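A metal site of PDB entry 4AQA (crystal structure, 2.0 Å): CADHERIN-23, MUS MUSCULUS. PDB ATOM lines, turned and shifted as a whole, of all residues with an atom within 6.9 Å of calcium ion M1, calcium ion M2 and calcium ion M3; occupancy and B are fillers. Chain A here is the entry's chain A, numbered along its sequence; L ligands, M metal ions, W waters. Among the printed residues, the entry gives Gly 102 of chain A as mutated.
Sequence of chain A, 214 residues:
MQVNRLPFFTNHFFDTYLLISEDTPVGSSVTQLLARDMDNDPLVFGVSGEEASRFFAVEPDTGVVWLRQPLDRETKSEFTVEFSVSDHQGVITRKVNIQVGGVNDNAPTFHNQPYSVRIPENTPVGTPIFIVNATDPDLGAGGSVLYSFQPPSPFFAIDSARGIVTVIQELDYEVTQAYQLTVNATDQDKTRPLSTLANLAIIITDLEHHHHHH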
ATOM      1  N   GLU A  22     -13.005  21.941  -4.266  1.00  0.00           N
ATOM      2  CA  GLU A  22     -13.675  20.651  -4.145  1.00  0.00           C
ATOM      3  C   GLU A  22     -12.913  19.538  -4.858  1.00  0.00           C
ATOM      4  O   GLU A  22     -13.195  18.359  -4.623  1.00  0.00           O
ATOM      5  CB  GLU A  22     -15.109  20.707  -4.660  1.00  0.00           C
ATOM      6  CG  GLU A  22     -15.264  20.901  -6.180  1.00  0.00           C
ATOM      7  CD  GLU A  22     -16.690  20.715  -6.660  1.00  0.00           C
ATOM      8  OE1 GLU A  22     -17.427  19.905  -6.063  1.00  0.00           O
ATOM      9  OE2 GLU A  22     -17.086  21.357  -7.670  1.00  0.00           O
ATOM     10  N   LEU A  71     -14.502  16.759  -0.592  1.00  0.00           N
ATOM     11  CA  LEU A  71     -15.511  17.812  -0.529  1.00  0.00           C
ATOM     12  C   LEU A  71     -16.334  17.775  -1.793  1.00  0.00           C
ATOM     13  O   LEU A  71     -15.947  17.170  -2.802  1.00  0.00           O
ATOM     14  CB  LEU A  71     -14.863  19.188  -0.374  1.00  0.00           C
ATOM     15  CG  LEU A  71     -13.934  19.327   0.825  1.00  0.00           C
ATOM     16  CD1 LEU A  71     -13.258  20.687   0.777  1.00  0.00           C
ATOM     17  CD2 LEU A  71     -14.700  19.127   2.126  1.00  0.00           C
ATOM     18  N   ASP A  72     -17.498  18.401  -1.743  1.00  0.00           N
ATOM     19  CA  ASP A  72     -18.371  18.477  -2.884  1.00  0.00           C
ATOM     20  C   ASP A  72     -19.168  19.762  -2.820  1.00  0.00           C
ATOM     21  O   ASP A  72     -20.103  19.875  -2.027  1.00  0.00           O
ATOM     22  CB  ASP A  72     -19.304  17.270  -2.923  1.00  0.00           C
ATOM     23  CG  ASP A  72     -20.220  17.285  -4.110  1.00  0.00           C
ATOM     24  OD1 ASP A  72     -20.131  18.245  -4.943  1.00  0.00           O
ATOM     25  OD2 ASP A  72     -21.043  16.346  -4.236  1.00  0.00           O
ATOM     26  N   ARG A  73     -18.819  20.728  -3.672  1.00  0.00           N
ATOM     27  CA  ARG A  73     -19.473  22.020  -3.669  1.00  0.00           C
ATOM     28  C   ARG A  73     -20.973  21.913  -3.958  1.00  0.00           C
ATOM     29  O   ARG A  73     -21.774  22.700  -3.442  1.00  0.00           O
ATOM     30  CB  ARG A  73     -18.817  22.947  -4.684  1.00  0.00           C
ATOM     31  CG  ARG A  73     -19.284  24.375  -4.548  1.00  0.00           C
ATOM     32  CD  ARG A  73     -19.368  25.054  -5.897  1.00  0.00           C
ATOM     33  NE  ARG A  73     -20.408  24.469  -6.716  1.00  0.00           N
ATOM     34  CZ  ARG A  73     -21.698  24.799  -6.664  1.00  0.00           C
ATOM     35  NH1 ARG A  73     -22.140  25.692  -5.770  1.00  0.00           N
ATOM     36  NH2 ARG A  73     -22.552  24.206  -7.472  1.00  0.00           N
ATOM     37  N   GLU A  74     -21.353  20.935  -4.775  1.00  0.00           N
ATOM     38  CA  GLU A  74     -22.755  20.750  -5.121  1.00  0.00           C
ATOM     39  C   GLU A  74     -23.583  20.331  -3.918  1.00  0.00           C
ATOM     40  O   GLU A  74     -24.770  20.621  -3.872  1.00  0.00           O
ATOM     41  CB  GLU A  74     -22.932  19.758  -6.281  1.00  0.00           C
ATOM     42  CG  GLU A  74     -22.669  20.347  -7.668  1.00  0.00           C
ATOM     43  CD  GLU A  74     -21.209  20.774  -7.871  1.00  0.00           C
ATOM     44  OE1 GLU A  74     -20.294  19.965  -7.578  1.00  0.00           O
ATOM     45  OE2 GLU A  74     -20.997  21.937  -8.344  1.00  0.00           O
ATOM     46  N   THR A  75     -22.960  19.660  -2.952  1.00  0.00           N
ATOM     47  CA  THR A  75     -23.643  19.260  -1.719  1.00  0.00           C
ATOM     48  C   THR A  75     -23.573  20.346  -0.643  1.00  0.00           C
ATOM     49  O   THR A  75     -24.560  20.611   0.025  1.00  0.00           O
ATOM     50  CB  THR A  75     -23.029  17.989  -1.133  1.00  0.00           C
ATOM     51  OG1 THR A  75     -23.077  16.946  -2.109  1.00  0.00           O
ATOM     52  CG2 THR A  75     -23.816  17.553   0.110  1.00  0.00           C
ATOM     53  N   GLY A 101     -14.482  25.596  -3.006  1.00  0.00           N
ATOM     54  CA  GLY A 101     -14.298  26.084  -4.366  1.00  0.00           C
ATOM     55  C   GLY A 101     -14.815  25.103  -5.401  1.00  0.00           C
ATOM     56  O   GLY A 101     -14.704  23.887  -5.207  1.00  0.00           O
ATOM     57  N   GLY A 102     -15.356  25.629  -6.496  1.00  0.00           N
ATOM     58  CA  GLY A 102     -16.022  24.848  -7.504  1.00  0.00           C
ATOM     59  C   GLY A 102     -15.088  24.474  -8.618  1.00  0.00           C
ATOM     60  O   GLY A 102     -14.151  25.190  -8.923  1.00  0.00           O
ATOM     61  N   VAL A 103     -15.295  23.277  -9.172  1.00  0.00           N
ATOM     62  CA  VAL A 103     -14.715  22.935 -10.464  1.00  0.00           C
ATOM     63  C   VAL A 103     -15.810  22.211 -11.227  1.00  0.00           C
ATOM     64  O   VAL A 103     -16.768  21.732 -10.653  1.00  0.00           O
ATOM     65  CB  VAL A 103     -13.500  21.987 -10.344  1.00  0.00           C
ATOM     66  CG1 VAL A 103     -12.438  22.530  -9.386  1.00  0.00           C
ATOM     67  CG2 VAL A 103     -13.951  20.592  -9.920  1.00  0.00           C
ATOM     68  N   ASN A 104     -15.670  22.124 -12.540  1.00  0.00           N
ATOM     69  CA  ASN A 104     -16.664  21.445 -13.348  1.00  0.00           C
ATOM     70  C   ASN A 104     -16.523  19.934 -13.160  1.00  0.00           C
ATOM     71  O   ASN A 104     -15.564  19.330 -13.670  1.00  0.00           O
ATOM     72  CB  ASN A 104     -16.503  21.811 -14.813  1.00  0.00           C
ATOM     73  CG  ASN A 104     -17.675  21.320 -15.648  1.00  0.00           C
ATOM     74  OD1 ASN A 104     -18.834  21.526 -15.281  1.00  0.00           O
ATOM     75  ND2 ASN A 104     -17.380  20.646 -16.757  1.00  0.00           N
ATOM     76  N   ASP A 105     -17.444  19.338 -12.406  1.00  0.00           N
ATOM     77  CA  ASP A 105     -17.415  17.882 -12.236  1.00  0.00           C
ATOM     78  C   ASP A 105     -18.731  17.147 -12.440  1.00  0.00           C
ATOM     79  O   ASP A 105     -18.838  15.966 -12.121  1.00  0.00           O
ATOM     80  CB  ASP A 105     -16.719  17.489 -10.915  1.00  0.00           C
ATOM     81  CG  ASP A 105     -17.387  18.049  -9.656  1.00  0.00           C
ATOM     82  OD1 ASP A 105     -18.295  18.918  -9.723  1.00  0.00           O
ATOM     83  OD2 ASP A 105     -16.975  17.616  -8.545  1.00  0.00           O
ATOM     84  N   ASN A 106     -19.730  17.800 -13.030  1.00  0.00           N
ATOM     85  CA  ASN A 106     -20.950  17.110 -13.460  1.00  0.00           C
ATOM     86  C   ASN A 106     -21.236  17.343 -14.935  1.00  0.00           C
ATOM     87  O   ASN A 106     -20.895  18.395 -15.471  1.00  0.00           O
ATOM     88  CB  ASN A 106     -22.170  17.579 -12.664  1.00  0.00           C
ATOM     89  CG  ASN A 106     -22.013  17.364 -11.170  1.00  0.00           C
ATOM     90  OD1 ASN A 106     -22.570  16.399 -10.632  1.00  0.00           O
ATOM     91  ND2 ASN A 106     -21.250  18.229 -10.486  1.00  0.00           N
ATOM     92  N   ALA A 107     -21.854  16.349 -15.573  1.00  0.00           N
ATOM     93  CA  ALA A 107     -22.333  16.521 -16.927  1.00  0.00           C
ATOM     94  C   ALA A 107     -23.784  16.916 -16.780  1.00  0.00           C
ATOM     95  O   ALA A 107     -24.328  16.728 -15.706  1.00  0.00           O
ATOM     96  CB  ALA A 107     -22.207  15.221 -17.714  1.00  0.00           C
ATOM     97  N   PRO A 108     -24.391  17.488 -17.823  1.00  0.00           N
ATOM     98  CA  PRO A 108     -25.832  17.765 -17.778  1.00  0.00           C
ATOM     99  C   PRO A 108     -26.710  16.520 -17.675  1.00  0.00           C
ATOM    100  O   PRO A 108     -26.285  15.423 -18.040  1.00  0.00           O
ATOM    101  CB  PRO A 108     -26.104  18.505 -19.090  1.00  0.00           C
ATOM    102  CG  PRO A 108     -24.775  19.000 -19.547  1.00  0.00           C
ATOM    103  CD  PRO A 108     -23.789  17.976 -19.080  1.00  0.00           C
ATOM    104  N   ASP A 136     -27.605  21.342 -15.250  1.00  0.00           N
ATOM    105  CA  ASP A 136     -26.239  21.002 -14.812  1.00  0.00           C
ATOM    106  C   ASP A 136     -25.964  21.834 -13.575  1.00  0.00           C
ATOM    107  O   ASP A 136     -26.078  23.037 -13.657  1.00  0.00           O
ATOM    108  CB  ASP A 136     -25.261  21.365 -15.918  1.00  0.00           C
ATOM    109  CG  ASP A 136     -23.835  20.914 -15.615  1.00  0.00           C
ATOM    110  OD1 ASP A 136     -23.359  21.047 -14.445  1.00  0.00           O
ATOM    111  OD2 ASP A 136     -23.180  20.426 -16.575  1.00  0.00           O
ATOM    112  N   PRO A 137     -25.596  21.200 -12.444  1.00  0.00           N
ATOM    113  CA  PRO A 137     -25.484  21.885 -11.150  1.00  0.00           C
ATOM    114  C   PRO A 137     -24.146  22.633 -10.868  1.00  0.00           C
ATOM    115  O   PRO A 137     -24.042  23.313  -9.859  1.00  0.00           O
ATOM    116  CB  PRO A 137     -25.662  20.741 -10.165  1.00  0.00           C
ATOM    117  CG  PRO A 137     -24.990  19.601 -10.862  1.00  0.00           C
ATOM    118  CD  PRO A 137     -25.358  19.756 -12.307  1.00  0.00           C
ATOM    119  N   ASP A 138     -23.168  22.519 -11.754  1.00  0.00           N
ATOM    120  CA  ASP A 138     -21.889  23.199 -11.546  1.00  0.00           C
ATOM    121  C   ASP A 138     -22.049  24.709 -11.719  1.00  0.00           C
ATOM    122  O   ASP A 138     -22.993  25.168 -12.352  1.00  0.00           O
ATOM    123  CB  ASP A 138     -20.811  22.693 -12.506  1.00  0.00           C
ATOM    124  CG  ASP A 138     -20.511  21.199 -12.343  1.00  0.00           C
ATOM    125  OD1 ASP A 138     -20.087  20.766 -11.224  1.00  0.00           O
ATOM    126  OD2 ASP A 138     -20.678  20.481 -13.349  1.00  0.00           O
ATOM    127  N   LEU A 139     -21.112  25.456 -11.147  1.00  0.00           N
ATOM    128  CA  LEU A 139     -21.142  26.909 -11.209  1.00  0.00           C
ATOM    129  C   LEU A 139     -20.779  27.415 -12.608  1.00  0.00           C
ATOM    130  O   LEU A 139     -19.941  26.822 -13.312  1.00  0.00           O
ATOM    131  CB  LEU A 139     -20.189  27.524 -10.191  1.00  0.00           C
ATOM    132  CG  LEU A 139     -20.562  27.467  -8.712  1.00  0.00           C
ATOM    133  CD1 LEU A 139     -19.533  28.241  -7.920  1.00  0.00           C
ATOM    134  CD2 LEU A 139     -21.950  28.041  -8.453  1.00  0.00           C
ATOM    135  N   ALA A 141     -19.907  28.730 -16.196  1.00  0.00           N
ATOM    136  CA  ALA A 141     -19.835  28.158 -17.530  1.00  0.00           C
ATOM    137  C   ALA A 141     -20.058  26.659 -17.469  1.00  0.00           C
ATOM    138  O   ALA A 141     -20.670  26.063 -18.356  1.00  0.00           O
ATOM    139  CB  ALA A 141     -18.501  28.486 -18.201  1.00  0.00           C
ATOM    140  N   GLY A 142     -19.555  26.044 -16.403  1.00  0.00           N
ATOM    141  CA  GLY A 142     -19.733  24.623 -16.216  1.00  0.00           C
ATOM    142  C   GLY A 142     -21.169  24.225 -15.951  1.00  0.00           C
ATOM    143  O   GLY A 142     -21.449  23.052 -15.932  1.00  0.00           O
ATOM    144  N   GLY A 143     -22.065  25.184 -15.741  1.00  0.00           N
ATOM    145  CA  GLY A 143     -23.461  24.892 -15.486  1.00  0.00           C
ATOM    146  C   GLY A 143     -24.406  25.385 -16.557  1.00  0.00           C
ATOM    147  O   GLY A 143     -25.625  25.237 -16.416  1.00  0.00           O
ATOM    148  N   SER A 144     -23.871  25.979 -17.633  1.00  0.00           N
ATOM    149  CA  SER A 144     -24.676  26.591 -18.674  1.00  0.00           C
ATOM    150  C   SER A 144     -24.672  25.658 -19.877  1.00  0.00           C
ATOM    151  O   SER A 144     -23.612  25.308 -20.403  1.00  0.00           O
ATOM    152  CB  SER A 144     -24.115  27.978 -19.019  1.00  0.00           C
ATOM    153  OG  SER A 144     -24.814  28.575 -20.117  1.00  0.00           O
ATOM    154  N   THR A 186     -24.157  19.817 -23.640  1.00  0.00           N
ATOM    155  CA  THR A 186     -22.824  20.049 -23.072  1.00  0.00           C
ATOM    156  C   THR A 186     -22.823  21.299 -22.218  1.00  0.00           C
ATOM    157  O   THR A 186     -23.540  22.289 -22.511  1.00  0.00           O
ATOM    158  CB  THR A 186     -21.692  20.169 -24.139  1.00  0.00           C
ATOM    159  OG1 THR A 186     -20.422  20.371 -23.484  1.00  0.00           O
ATOM    160  CG2 THR A 186     -21.896  21.350 -25.073  1.00  0.00           C
ATOM    161  N   ASP A 187     -22.041  21.259 -21.157  1.00  0.00           N
ATOM    162  CA  ASP A 187     -21.713  22.501 -20.459  1.00  0.00           C
ATOM    163  C   ASP A 187     -20.612  23.220 -21.235  1.00  0.00           C
ATOM    164  O   ASP A 187     -20.160  22.747 -22.289  1.00  0.00           O
ATOM    165  CB  ASP A 187     -21.409  22.290 -18.973  1.00  0.00           C
ATOM    166  CG  ASP A 187     -20.175  21.406 -18.728  1.00  0.00           C
ATOM    167  OD1 ASP A 187     -19.196  21.542 -19.471  1.00  0.00           O
ATOM    168  OD2 ASP A 187     -20.230  20.594 -17.768  1.00  0.00           O
ATOM    169  N   GLN A 188     -20.259  24.406 -20.759  1.00  0.00           N
ATOM    170  CA  GLN A 188     -19.316  25.268 -21.433  1.00  0.00           C
ATOM    171  C   GLN A 188     -18.041  25.506 -20.620  1.00  0.00           C
ATOM    172  O   GLN A 188     -17.398  26.506 -20.801  1.00  0.00           O
ATOM    173  CB  GLN A 188     -19.997  26.603 -21.717  1.00  0.00           C
ATOM    174  CG  GLN A 188     -21.082  26.485 -22.755  1.00  0.00           C
ATOM    175  CD  GLN A 188     -21.772  27.784 -23.025  1.00  0.00           C
ATOM    176  OE1 GLN A 188     -21.357  28.549 -23.899  1.00  0.00           O
ATOM    177  NE2 GLN A 188     -22.844  28.055 -22.279  1.00  0.00           N
ATOM    178  N   ASP A 189     -17.673  24.592 -19.740  1.00  0.00           N
ATOM    179  CA  ASP A 189     -16.424  24.769 -19.020  1.00  0.00           C
ATOM    180  C   ASP A 189     -15.286  24.902 -20.050  1.00  0.00           C
ATOM    181  O   ASP A 189     -15.297  24.225 -21.078  1.00  0.00           O
ATOM    182  CB  ASP A 189     -16.163  23.578 -18.104  1.00  0.00           C
ATOM    183  CG  ASP A 189     -14.992  23.822 -17.199  1.00  0.00           C
ATOM    184  OD1 ASP A 189     -15.052  24.753 -16.358  1.00  0.00           O
ATOM    185  OD2 ASP A 189     -14.004  23.076 -17.304  1.00  0.00           O
ATOM    186  N   ARG A 192     -12.442  21.572 -19.175  1.00  0.00           N
ATOM    187  CA  ARG A 192     -12.978  20.214 -19.089  1.00  0.00           C
ATOM    188  C   ARG A 192     -14.497  20.203 -19.310  1.00  0.00           C
ATOM    189  O   ARG A 192     -15.253  19.940 -18.374  1.00  0.00           O
ATOM    190  CB  ARG A 192     -12.639  19.585 -17.730  1.00  0.00           C
ATOM    191  CG  ARG A 192     -11.145  19.462 -17.473  1.00  0.00           C
ATOM    192  CD  ARG A 192     -10.782  18.846 -16.122  1.00  0.00           C
ATOM    193  NE  ARG A 192     -11.360  17.511 -16.004  1.00  0.00           N
ATOM    194  CZ  ARG A 192     -12.503  17.207 -15.378  1.00  0.00           C
ATOM    195  NH1 ARG A 192     -13.226  18.122 -14.758  1.00  0.00           N
ATOM    196  NH2 ARG A 192     -12.928  15.946 -15.399  1.00  0.00           N
ATOM    197  N   PRO A 193     -14.951  20.493 -20.536  1.00  0.00           N
ATOM    198  CA  PRO A 193     -16.395  20.451 -20.761  1.00  0.00           C
ATOM    199  C   PRO A 193     -16.920  19.018 -20.664  1.00  0.00           C
ATOM    200  O   PRO A 193     -16.207  18.044 -21.006  1.00  0.00           O
ATOM    201  CB  PRO A 193     -16.564  20.998 -22.168  1.00  0.00           C
ATOM    202  CG  PRO A 193     -15.270  20.670 -22.831  1.00  0.00           C
ATOM    203  CD  PRO A 193     -14.221  20.837 -21.771  1.00  0.00           C
ATOM    204  N   LEU A 194     -18.149  18.896 -20.166  1.00  0.00           N
ATOM    205  CA  LEU A 194     -18.757  17.611 -19.962  1.00  0.00           C
ATOM    206  C   LEU A 194     -20.103  17.596 -20.663  1.00  0.00           C
ATOM    207  O   LEU A 194     -20.775  18.635 -20.735  1.00  0.00           O
ATOM    208  CB  LEU A 194     -18.895  17.314 -18.471  1.00  0.00           C
ATOM    209  CG  LEU A 194     -17.587  17.092 -17.696  1.00  0.00           C
ATOM    210  CD1 LEU A 194     -17.862  16.939 -16.204  1.00  0.00           C
ATOM    211  CD2 LEU A 194     -16.846  15.878 -18.222  1.00  0.00           C
HETATM  212 CL1  LIG L   1     -18.664  24.068  -9.622  1.00  0.00          CL
HETATM  213 CA    CA M   1     -21.086  20.736 -15.610  1.00  0.00          CA
HETATM  214 CA    CA M   2     -18.695  21.271  -9.356  1.00  0.00          CA
HETATM  215 CA    CA M   3     -18.745  18.236  -7.096  1.00  0.00          CA
HETATM  216  O   HOH W   1     -20.133  16.740  -8.065  1.00  0.00           O
HETATM  217  O   HOH W   2     -17.704  16.367  -5.947  1.00  0.00           O
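The side-chain carboxylate (OE1) of Glu 22 lies close to the backbone NH (N) of Arg 73, at 2.9 Å.
N of Glu 22 lies within hydrogen-bond range of O of Gly 101 (2.7 Å).
The side-chain amide nitrogen (ND2) of Asn 104 lies within hydrogen-bond range of the backbone carbonyl oxygen (O) of Arg 192 (2.8 Å).
OD1 of Asp 187 sits at hydrogen-bond distance from N of Leu 194, 2.9 Å away.
OE2 of Glu 74 lies close to NH2 of Arg 73.
OD1 of Asp 187 is in hydrogen-bond range of N of Asp 189 (3.4 Å).
OD2 of Asp 72 is in hydrogen-bond range of OG1 of Thr 75.
ND2 of Asn 106 lies close to OD1 of Asp 105, at 3.1 Å.
Calcium ion M2 is bound by OE2 of Glu 22 (2.3 Å), O of Val 103 (2.4 Å), OD1 of Asp 138 (2.4 Å), OD1 of Asp 105 (2.4 Å), OE2 of Glu 74 (2.6 Å), OE1 of Glu 74 (2.7 Å) and CL1 of the ligand (2.8 Å).
Calcium ion M3 is bound by water W1, OE1 of Glu 22, OE1 of Glu 74, OD2 of Asp 105, water W2, OD1 of Asp 72 and OD1 of Asp 105.
Along chain A the residues within 4 Å of calcium ion M3 span positions 22 to 105.
Calcium ion M1 is bound by OD2 of Asp 138 (2.3 Å), OD2 of Asp 136 (2.3 Å), OD2 of Asp 187 (2.3 Å), O of Asn 106 (2.4 Å), O of Gly 142 (2.4 Å), OD1 of Asn 104 (2.4 Å) and OD1 of Asp 136 (2.6 Å).
Calcium ion M1 has seven donor atoms within binding distance.
Six residues have an atom within 4 Å of calcium ion M1: Asn 104, Asn 106, Asp 136, Asp 138, Gly 142 and Asp 187.
The nearest printed residue that does not touch calcium ion M1 is Ala 107 (4.5 Å).
Five residues have an atom within 4 Å of calcium ion M2: Glu 22, Glu 74, Val 103, Asp 105 and Asp 138.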
